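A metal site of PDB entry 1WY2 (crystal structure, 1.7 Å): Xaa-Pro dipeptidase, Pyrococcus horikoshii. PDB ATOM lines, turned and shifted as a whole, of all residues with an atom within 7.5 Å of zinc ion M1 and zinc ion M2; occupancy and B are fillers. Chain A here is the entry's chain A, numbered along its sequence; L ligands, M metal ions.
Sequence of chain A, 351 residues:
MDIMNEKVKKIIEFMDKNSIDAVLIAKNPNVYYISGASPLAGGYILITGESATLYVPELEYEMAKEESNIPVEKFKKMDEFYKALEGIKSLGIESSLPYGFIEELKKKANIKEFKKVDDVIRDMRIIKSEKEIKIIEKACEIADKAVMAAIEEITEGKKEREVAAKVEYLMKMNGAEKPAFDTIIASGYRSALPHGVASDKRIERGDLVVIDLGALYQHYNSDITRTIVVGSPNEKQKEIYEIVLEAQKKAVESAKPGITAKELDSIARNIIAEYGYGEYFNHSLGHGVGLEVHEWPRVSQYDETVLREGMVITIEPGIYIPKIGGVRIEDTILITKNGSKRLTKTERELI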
ATOM      1  N   PHE A 181      33.623  11.257   6.807  1.00  0.00           N
ATOM      2  CA  PHE A 181      32.360  11.591   7.423  1.00  0.00           C
ATOM      3  C   PHE A 181      32.026  10.494   8.432  1.00  0.00           C
ATOM      4  O   PHE A 181      32.663   9.455   8.440  1.00  0.00           O
ATOM      5  CB  PHE A 181      31.263  11.700   6.347  1.00  0.00           C
ATOM      6  CG  PHE A 181      31.155  10.489   5.466  1.00  0.00           C
ATOM      7  CD1 PHE A 181      30.394   9.400   5.847  1.00  0.00           C
ATOM      8  CD2 PHE A 181      31.837  10.446   4.245  1.00  0.00           C
ATOM      9  CE1 PHE A 181      30.290   8.275   5.033  1.00  0.00           C
ATOM     10  CE2 PHE A 181      31.739   9.319   3.418  1.00  0.00           C
ATOM     11  CZ  PHE A 181      30.973   8.237   3.803  1.00  0.00           C
ATOM     12  N   ILE A 184      28.753   5.042   8.556  1.00  0.00           N
ATOM     13  CA  ILE A 184      27.428   4.463   8.626  1.00  0.00           C
ATOM     14  C   ILE A 184      27.510   2.940   8.598  1.00  0.00           C
ATOM     15  O   ILE A 184      28.032   2.362   7.653  1.00  0.00           O
ATOM     16  CB  ILE A 184      26.563   4.943   7.438  1.00  0.00           C
ATOM     17  CG1 ILE A 184      26.201   6.413   7.620  1.00  0.00           C
ATOM     18  CG2 ILE A 184      25.299   4.077   7.308  1.00  0.00           C
ATOM     19  CD1 ILE A 184      25.657   7.078   6.376  1.00  0.00           C
ATOM     20  N   HIS A 195      20.993   7.792   6.277  1.00  0.00           N
ATOM     21  CA  HIS A 195      22.125   8.278   7.056  1.00  0.00           C
ATOM     22  C   HIS A 195      22.176   7.678   8.461  1.00  0.00           C
ATOM     23  O   HIS A 195      22.426   8.382   9.438  1.00  0.00           O
ATOM     24  CB  HIS A 195      22.085   9.806   7.150  1.00  0.00           C
ATOM     25  CG  HIS A 195      22.445  10.501   5.867  1.00  0.00           C
ATOM     26  ND1 HIS A 195      22.235  11.841   5.661  1.00  0.00           N
ATOM     27  CD2 HIS A 195      23.008  10.021   4.726  1.00  0.00           C
ATOM     28  CE1 HIS A 195      22.655  12.173   4.450  1.00  0.00           C
ATOM     29  NE2 HIS A 195      23.129  11.077   3.862  1.00  0.00           N
ATOM     30  N   ILE A 211      26.899  -0.336   4.696  1.00  0.00           N
ATOM     31  CA  ILE A 211      28.202   0.167   5.134  1.00  0.00           C
ATOM     32  C   ILE A 211      28.596   1.332   4.221  1.00  0.00           C
ATOM     33  O   ILE A 211      28.942   1.125   3.067  1.00  0.00           O
ATOM     34  CB  ILE A 211      29.274  -0.940   5.009  1.00  0.00           C
ATOM     35  CG1 ILE A 211      28.813  -2.190   5.779  1.00  0.00           C
ATOM     36  CG2 ILE A 211      30.605  -0.443   5.564  1.00  0.00           C
ATOM     37  CD1 ILE A 211      29.565  -3.452   5.396  1.00  0.00           C
ATOM     38  N   ASP A 212      28.522   2.551   4.746  1.00  0.00           N
ATOM     39  CA  ASP A 212      28.848   3.759   3.984  1.00  0.00           C
ATOM     40  C   ASP A 212      29.962   4.469   4.749  1.00  0.00           C
ATOM     41  O   ASP A 212      29.770   4.911   5.887  1.00  0.00           O
ATOM     42  CB  ASP A 212      27.605   4.652   3.875  1.00  0.00           C
ATOM     43  CG  ASP A 212      27.747   5.753   2.840  1.00  0.00           C
ATOM     44  OD1 ASP A 212      28.884   6.125   2.480  1.00  0.00           O
ATOM     45  OD2 ASP A 212      26.702   6.275   2.397  1.00  0.00           O
ATOM     46  N   LEU A 213      31.128   4.588   4.137  1.00  0.00           N
ATOM     47  CA  LEU A 213      32.257   5.217   4.780  1.00  0.00           C
ATOM     48  C   LEU A 213      33.174   5.871   3.772  1.00  0.00           C
ATOM     49  O   LEU A 213      32.980   5.742   2.557  1.00  0.00           O
ATOM     50  CB  LEU A 213      33.033   4.162   5.598  1.00  0.00           C
ATOM     51  CG  LEU A 213      33.581   2.943   4.844  1.00  0.00           C
ATOM     52  CD1 LEU A 213      34.897   3.295   4.168  1.00  0.00           C
ATOM     53  CD2 LEU A 213      33.801   1.785   5.830  1.00  0.00           C
ATOM     54  N   GLY A 214      34.173   6.602   4.266  1.00  0.00           N
ATOM     55  CA  GLY A 214      35.095   7.254   3.363  1.00  0.00           C
ATOM     56  C   GLY A 214      36.319   7.729   4.131  1.00  0.00           C
ATOM     57  O   GLY A 214      36.268   7.872   5.355  1.00  0.00           O
ATOM     58  N   SER A 222      37.045  10.310  -0.222  1.00  0.00           N
ATOM     59  CA  SER A 222      36.600   9.104  -0.905  1.00  0.00           C
ATOM     60  C   SER A 222      35.229   8.785  -0.308  1.00  0.00           C
ATOM     61  O   SER A 222      34.893   9.248   0.783  1.00  0.00           O
ATOM     62  CB  SER A 222      37.572   7.945  -0.681  1.00  0.00           C
ATOM     63  OG  SER A 222      37.789   7.713   0.699  1.00  0.00           O
ATOM     64  N   ASP A 223      34.434   7.987  -1.004  1.00  0.00           N
ATOM     65  CA  ASP A 223      33.086   7.679  -0.540  1.00  0.00           C
ATOM     66  C   ASP A 223      32.660   6.353  -1.155  1.00  0.00           C
ATOM     67  O   ASP A 223      32.719   6.184  -2.370  1.00  0.00           O
ATOM     68  CB  ASP A 223      32.152   8.817  -0.987  1.00  0.00           C
ATOM     69  CG  ASP A 223      30.828   8.821  -0.265  1.00  0.00           C
ATOM     70  OD1 ASP A 223      30.538   7.873   0.510  1.00  0.00           O
ATOM     71  OD2 ASP A 223      30.071   9.790  -0.483  1.00  0.00           O
ATOM     72  N   ILE A 224      32.224   5.415  -0.316  1.00  0.00           N
ATOM     73  CA  ILE A 224      31.805   4.112  -0.797  1.00  0.00           C
ATOM     74  C   ILE A 224      30.722   3.498   0.080  1.00  0.00           C
ATOM     75  O   ILE A 224      30.703   3.715   1.282  1.00  0.00           O
ATOM     76  CB  ILE A 224      33.019   3.146  -0.855  1.00  0.00           C
ATOM     77  CG1 ILE A 224      32.625   1.805  -1.477  1.00  0.00           C
ATOM     78  CG2 ILE A 224      33.565   2.912   0.553  1.00  0.00           C
ATOM     79  CD1 ILE A 224      33.783   0.803  -1.587  1.00  0.00           C
ATOM     80  N   THR A 225      29.799   2.754  -0.534  1.00  0.00           N
ATOM     81  CA  THR A 225      28.742   2.073   0.207  1.00  0.00           C
ATOM     82  C   THR A 225      28.558   0.678  -0.346  1.00  0.00           C
ATOM     83  O   THR A 225      28.437   0.489  -1.555  1.00  0.00           O
ATOM     84  CB  THR A 225      27.353   2.764   0.112  1.00  0.00           C
ATOM     85  OG1 THR A 225      27.424   4.101   0.606  1.00  0.00           O
ATOM     86  CG2 THR A 225      26.324   1.998   0.945  1.00  0.00           C
ATOM     87  N   LEU A 285      20.955  10.697  -6.932  1.00  0.00           N
ATOM     88  CA  LEU A 285      21.786   9.576  -7.325  1.00  0.00           C
ATOM     89  C   LEU A 285      23.223   9.727  -6.836  1.00  0.00           C
ATOM     90  O   LEU A 285      23.904   8.732  -6.570  1.00  0.00           O
ATOM     91  CB  LEU A 285      21.802   9.432  -8.849  1.00  0.00           C
ATOM     92  CG  LEU A 285      22.681   8.309  -9.393  1.00  0.00           C
ATOM     93  CD1 LEU A 285      22.194   6.963  -8.864  1.00  0.00           C
ATOM     94  CD2 LEU A 285      22.665   8.328 -10.912  1.00  0.00           C
ATOM     95  N   GLY A 286      23.702  10.960  -6.725  1.00  0.00           N
ATOM     96  CA  GLY A 286      25.066  11.151  -6.277  1.00  0.00           C
ATOM     97  C   GLY A 286      25.510  12.575  -6.097  1.00  0.00           C
ATOM     98  O   GLY A 286      24.716  13.511  -6.208  1.00  0.00           O
ATOM     99  N   HIS A 287      26.799  12.746  -5.823  1.00  0.00           N
ATOM    100  CA  HIS A 287      27.374  14.063  -5.579  1.00  0.00           C
ATOM    101  C   HIS A 287      28.842  14.077  -5.968  1.00  0.00           C
ATOM    102  O   HIS A 287      29.487  13.026  -6.026  1.00  0.00           O
ATOM    103  CB  HIS A 287      27.244  14.401  -4.085  1.00  0.00           C
ATOM    104  CG  HIS A 287      27.830  13.355  -3.185  1.00  0.00           C
ATOM    105  ND1 HIS A 287      29.180  13.298  -2.883  1.00  0.00           N
ATOM    106  CD2 HIS A 287      27.265  12.288  -2.581  1.00  0.00           C
ATOM    107  CE1 HIS A 287      29.409  12.238  -2.131  1.00  0.00           C
ATOM    108  NE2 HIS A 287      28.261  11.604  -1.937  1.00  0.00           N
ATOM    109  N   GLY A 288      29.370  15.259  -6.253  1.00  0.00           N
ATOM    110  CA  GLY A 288      30.768  15.358  -6.595  1.00  0.00           C
ATOM    111  C   GLY A 288      31.597  15.129  -5.347  1.00  0.00           C
ATOM    112  O   GLY A 288      31.090  15.260  -4.232  1.00  0.00           O
ATOM    113  N   VAL A 289      32.864  14.756  -5.536  1.00  0.00           N
ATOM    114  CA  VAL A 289      33.777  14.492  -4.432  1.00  0.00           C
ATOM    115  C   VAL A 289      35.126  15.141  -4.740  1.00  0.00           C
ATOM    116  O   VAL A 289      35.593  15.120  -5.885  1.00  0.00           O
ATOM    117  CB  VAL A 289      34.004  12.968  -4.258  1.00  0.00           C
ATOM    118  CG1 VAL A 289      35.039  12.726  -3.164  1.00  0.00           C
ATOM    119  CG2 VAL A 289      32.691  12.276  -3.902  1.00  0.00           C
ATOM    120  N   VAL A 293      33.578  16.111   0.816  1.00  0.00           N
ATOM    121  CA  VAL A 293      32.904  14.876   0.425  1.00  0.00           C
ATOM    122  C   VAL A 293      31.661  15.152  -0.416  1.00  0.00           C
ATOM    123  O   VAL A 293      31.282  14.333  -1.253  1.00  0.00           O
ATOM    124  CB  VAL A 293      32.549  14.011   1.661  1.00  0.00           C
ATOM    125  CG1 VAL A 293      31.359  14.577   2.383  1.00  0.00           C
ATOM    126  CG2 VAL A 293      32.295  12.567   1.226  1.00  0.00           C
ATOM    127  N   HIS A 294      31.040  16.313  -0.192  1.00  0.00           N
ATOM    128  CA  HIS A 294      29.872  16.724  -0.966  1.00  0.00           C
ATOM    129  C   HIS A 294      30.200  18.020  -1.719  1.00  0.00           C
ATOM    130  O   HIS A 294      30.304  19.081  -1.099  1.00  0.00           O
ATOM    131  CB  HIS A 294      28.665  17.000  -0.061  1.00  0.00           C
ATOM    132  CG  HIS A 294      28.091  15.776   0.572  1.00  0.00           C
ATOM    133  ND1 HIS A 294      28.148  15.554   1.931  1.00  0.00           N
ATOM    134  CD2 HIS A 294      27.432  14.721   0.047  1.00  0.00           C
ATOM    135  CE1 HIS A 294      27.543  14.414   2.212  1.00  0.00           C
ATOM    136  NE2 HIS A 294      27.102  13.892   1.083  1.00  0.00           N
ATOM    137  N   THR A 314      29.849  10.470  -7.273  1.00  0.00           N
ATOM    138  CA  THR A 314      29.450   9.180  -6.736  1.00  0.00           C
ATOM    139  C   THR A 314      28.171   8.768  -7.470  1.00  0.00           C
ATOM    140  O   THR A 314      27.456   9.608  -8.002  1.00  0.00           O
ATOM    141  CB  THR A 314      29.127   9.244  -5.231  1.00  0.00           C
ATOM    142  OG1 THR A 314      28.032  10.147  -5.012  1.00  0.00           O
ATOM    143  CG2 THR A 314      30.339   9.693  -4.432  1.00  0.00           C
ATOM    144  N   ILE A 315      27.935   7.466  -7.518  1.00  0.00           N
ATOM    145  CA  ILE A 315      26.742   6.896  -8.130  1.00  0.00           C
ATOM    146  C   ILE A 315      26.255   5.998  -6.998  1.00  0.00           C
ATOM    147  O   ILE A 315      26.853   4.960  -6.709  1.00  0.00           O
ATOM    148  CB  ILE A 315      27.101   6.038  -9.373  1.00  0.00           C
ATOM    149  CG1 ILE A 315      27.757   6.921 -10.440  1.00  0.00           C
ATOM    150  CG2 ILE A 315      25.847   5.385  -9.937  1.00  0.00           C
ATOM    151  CD1 ILE A 315      26.862   8.033 -10.960  1.00  0.00           C
ATOM    152  N   GLU A 316      25.175   6.409  -6.341  1.00  0.00           N
ATOM    153  CA  GLU A 316      24.701   5.646  -5.194  1.00  0.00           C
ATOM    154  C   GLU A 316      23.196   5.516  -5.023  1.00  0.00           C
ATOM    155  O   GLU A 316      22.617   6.073  -4.085  1.00  0.00           O
ATOM    156  CB  GLU A 316      25.295   6.244  -3.919  1.00  0.00           C
ATOM    157  CG  GLU A 316      25.027   7.744  -3.745  1.00  0.00           C
ATOM    158  CD  GLU A 316      25.706   8.314  -2.505  1.00  0.00           C
ATOM    159  OE1 GLU A 316      25.544   7.732  -1.416  1.00  0.00           O
ATOM    160  OE2 GLU A 316      26.391   9.352  -2.629  1.00  0.00           O
ATOM    161  N   ARG A 328      21.846   0.112  -0.350  1.00  0.00           N
ATOM    162  CA  ARG A 328      22.524   1.173  -1.089  1.00  0.00           C
ATOM    163  C   ARG A 328      23.872   0.646  -1.570  1.00  0.00           C
ATOM    164  O   ARG A 328      24.579  -0.051  -0.829  1.00  0.00           O
ATOM    165  CB  ARG A 328      22.752   2.430  -0.239  1.00  0.00           C
ATOM    166  CG  ARG A 328      23.528   3.513  -1.015  1.00  0.00           C
ATOM    167  CD  ARG A 328      23.472   4.919  -0.370  1.00  0.00           C
ATOM    168  NE  ARG A 328      24.130   5.009   0.933  1.00  0.00           N
ATOM    169  CZ  ARG A 328      23.506   4.921   2.101  1.00  0.00           C
ATOM    170  NH1 ARG A 328      22.201   4.748   2.144  1.00  0.00           N
ATOM    171  NH2 ARG A 328      24.194   5.061   3.237  1.00  0.00           N
ATOM    172  N   GLU A 330      27.216   2.225  -3.526  1.00  0.00           N
ATOM    173  CA  GLU A 330      27.849   3.457  -3.959  1.00  0.00           C
ATOM    174  C   GLU A 330      29.307   3.348  -4.356  1.00  0.00           C
ATOM    175  O   GLU A 330      30.095   2.694  -3.664  1.00  0.00           O
ATOM    176  CB  GLU A 330      27.719   4.502  -2.838  1.00  0.00           C
ATOM    177  CG  GLU A 330      28.662   5.701  -2.978  1.00  0.00           C
ATOM    178  CD  GLU A 330      28.541   6.691  -1.844  1.00  0.00           C
ATOM    179  OE1 GLU A 330      28.369   6.252  -0.689  1.00  0.00           O
ATOM    180  OE2 GLU A 330      28.661   7.898  -2.103  1.00  0.00           O
ATOM    181  N   ASP A 331      29.656   3.982  -5.477  1.00  0.00           N
ATOM    182  CA  ASP A 331      31.035   4.019  -5.967  1.00  0.00           C
ATOM    183  C   ASP A 331      31.407   5.469  -6.204  1.00  0.00           C
ATOM    184  O   ASP A 331      30.540   6.302  -6.458  1.00  0.00           O
ATOM    185  CB  ASP A 331      31.191   3.313  -7.323  1.00  0.00           C
ATOM    186  CG  ASP A 331      31.355   1.819  -7.207  1.00  0.00           C
ATOM    187  OD1 ASP A 331      32.123   1.358  -6.335  1.00  0.00           O
ATOM    188  OD2 ASP A 331      30.733   1.102  -8.024  1.00  0.00           O
ATOM    189  N   THR A 332      32.697   5.779  -6.103  1.00  0.00           N
ATOM    190  CA  THR A 332      33.180   7.113  -6.426  1.00  0.00           C
ATOM    191  C   THR A 332      33.755   6.832  -7.807  1.00  0.00           C
ATOM    192  O   THR A 332      34.500   5.858  -7.974  1.00  0.00           O
ATOM    193  CB  THR A 332      34.305   7.591  -5.499  1.00  0.00           C
ATOM    194  OG1 THR A 332      33.767   7.870  -4.210  1.00  0.00           O
ATOM    195  CG2 THR A 332      34.967   8.857  -6.050  1.00  0.00           C
HETATM  196 AS1  LIG L   1      27.270  10.214   1.933  1.00  0.00          AS
HETATM  197  O1  LIG L   1      27.499   9.093   0.738  1.00  0.00           O
HETATM  198  O2  LIG L   1      26.203  11.300   1.346  1.00  0.00           O
HETATM  199  C1  LIG L   1      26.507   9.453   3.458  1.00  0.00           C
HETATM  200  C2  LIG L   1      28.842  11.170   2.278  1.00  0.00           C
HETATM  201 ZN    ZN M   1      28.638   7.385   0.927  1.00  0.00          ZN
HETATM  202 ZN    ZN M   2      28.064   9.663  -1.163  1.00  0.00          ZN
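Zinc ion M1 is bound by OE1 of Glu 330 (2.0 Å), OD1 of Asp 223 (2.0 Å), OD1 of Asp 212 (2.0 Å) and O1 of the ligand (2.1 Å).
Slightly farther from zinc ion M1 lies the side-chain carboxylate (OD2) of Asp 212 (2.7 Å).
Residues that only touch zinc ion M2: Thr 314.
Five residues have an atom within 4 Å of zinc ion M2: Asp 223, His 287, Thr 314, Glu 316 and Glu 330.
Along chain A the residues within 4 Å of zinc ion M2 span positions 223 to 330.
The nearest printed residue that does not touch zinc ion M2 is His 294 (4.9 Å).
The backbone NH (N) of Glu 330 is in hydrogen-bond range of the backbone carbonyl oxygen (O) of Thr 225.
The side-chain hydroxyl of Thr 225 lies close to the side-chain carboxylate of Asp 212, 2.9 Å away.
OD2 of Asp 212 is in salt-bridge range of NH2 of Arg 328, at 2.9 Å.
O of Asp 212 lies within hydrogen-bond range of N of Ile 184 (2.9 Å).
The backbone NH (N) of Thr 314 is in hydrogen-bond range of the backbone carbonyl oxygen (O) of His 287, at 2.9 Å.
The backbone carbonyl oxygen (O) of Val 293 lies within hydrogen-bond range of a ring nitrogen (ND1) of His 287 (2.9 Å).
OE2 of Glu 316 lies close to OG1 of Thr 314, at 3.0 Å.
The guanidinium group (NE) of Arg 328 sits at hydrogen-bond distance from the side-chain hydroxyl (OG1) of Thr 225.
O1 of the ligand binds zinc ion M2 (2.1 Å).
OE2 of Glu 330 binds zinc ion M2 (2.1 Å).
Zinc ion M2 is bound by NE2 of His 287 (2.1 Å).
OD2 of Asp 223 is bound to zinc ion M2, at 2.1 Å.
OE2 of Glu 316 is bound to zinc ion M2, 2.2 Å away.
Zinc ion M2 has five donor atoms within binding distance.
CZ of Phe 181 touches zinc ion M1, 3.8 Å away.
Thr 225 touches zinc ion M1.
Within 4 Å of zinc ion M1: Phe 181, Asp 212, Asp 223, Thr 225, Glu 316 and Glu 330.
Along chain A the residues within 4 Å of zinc ion M1 span positions 181 to 330.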
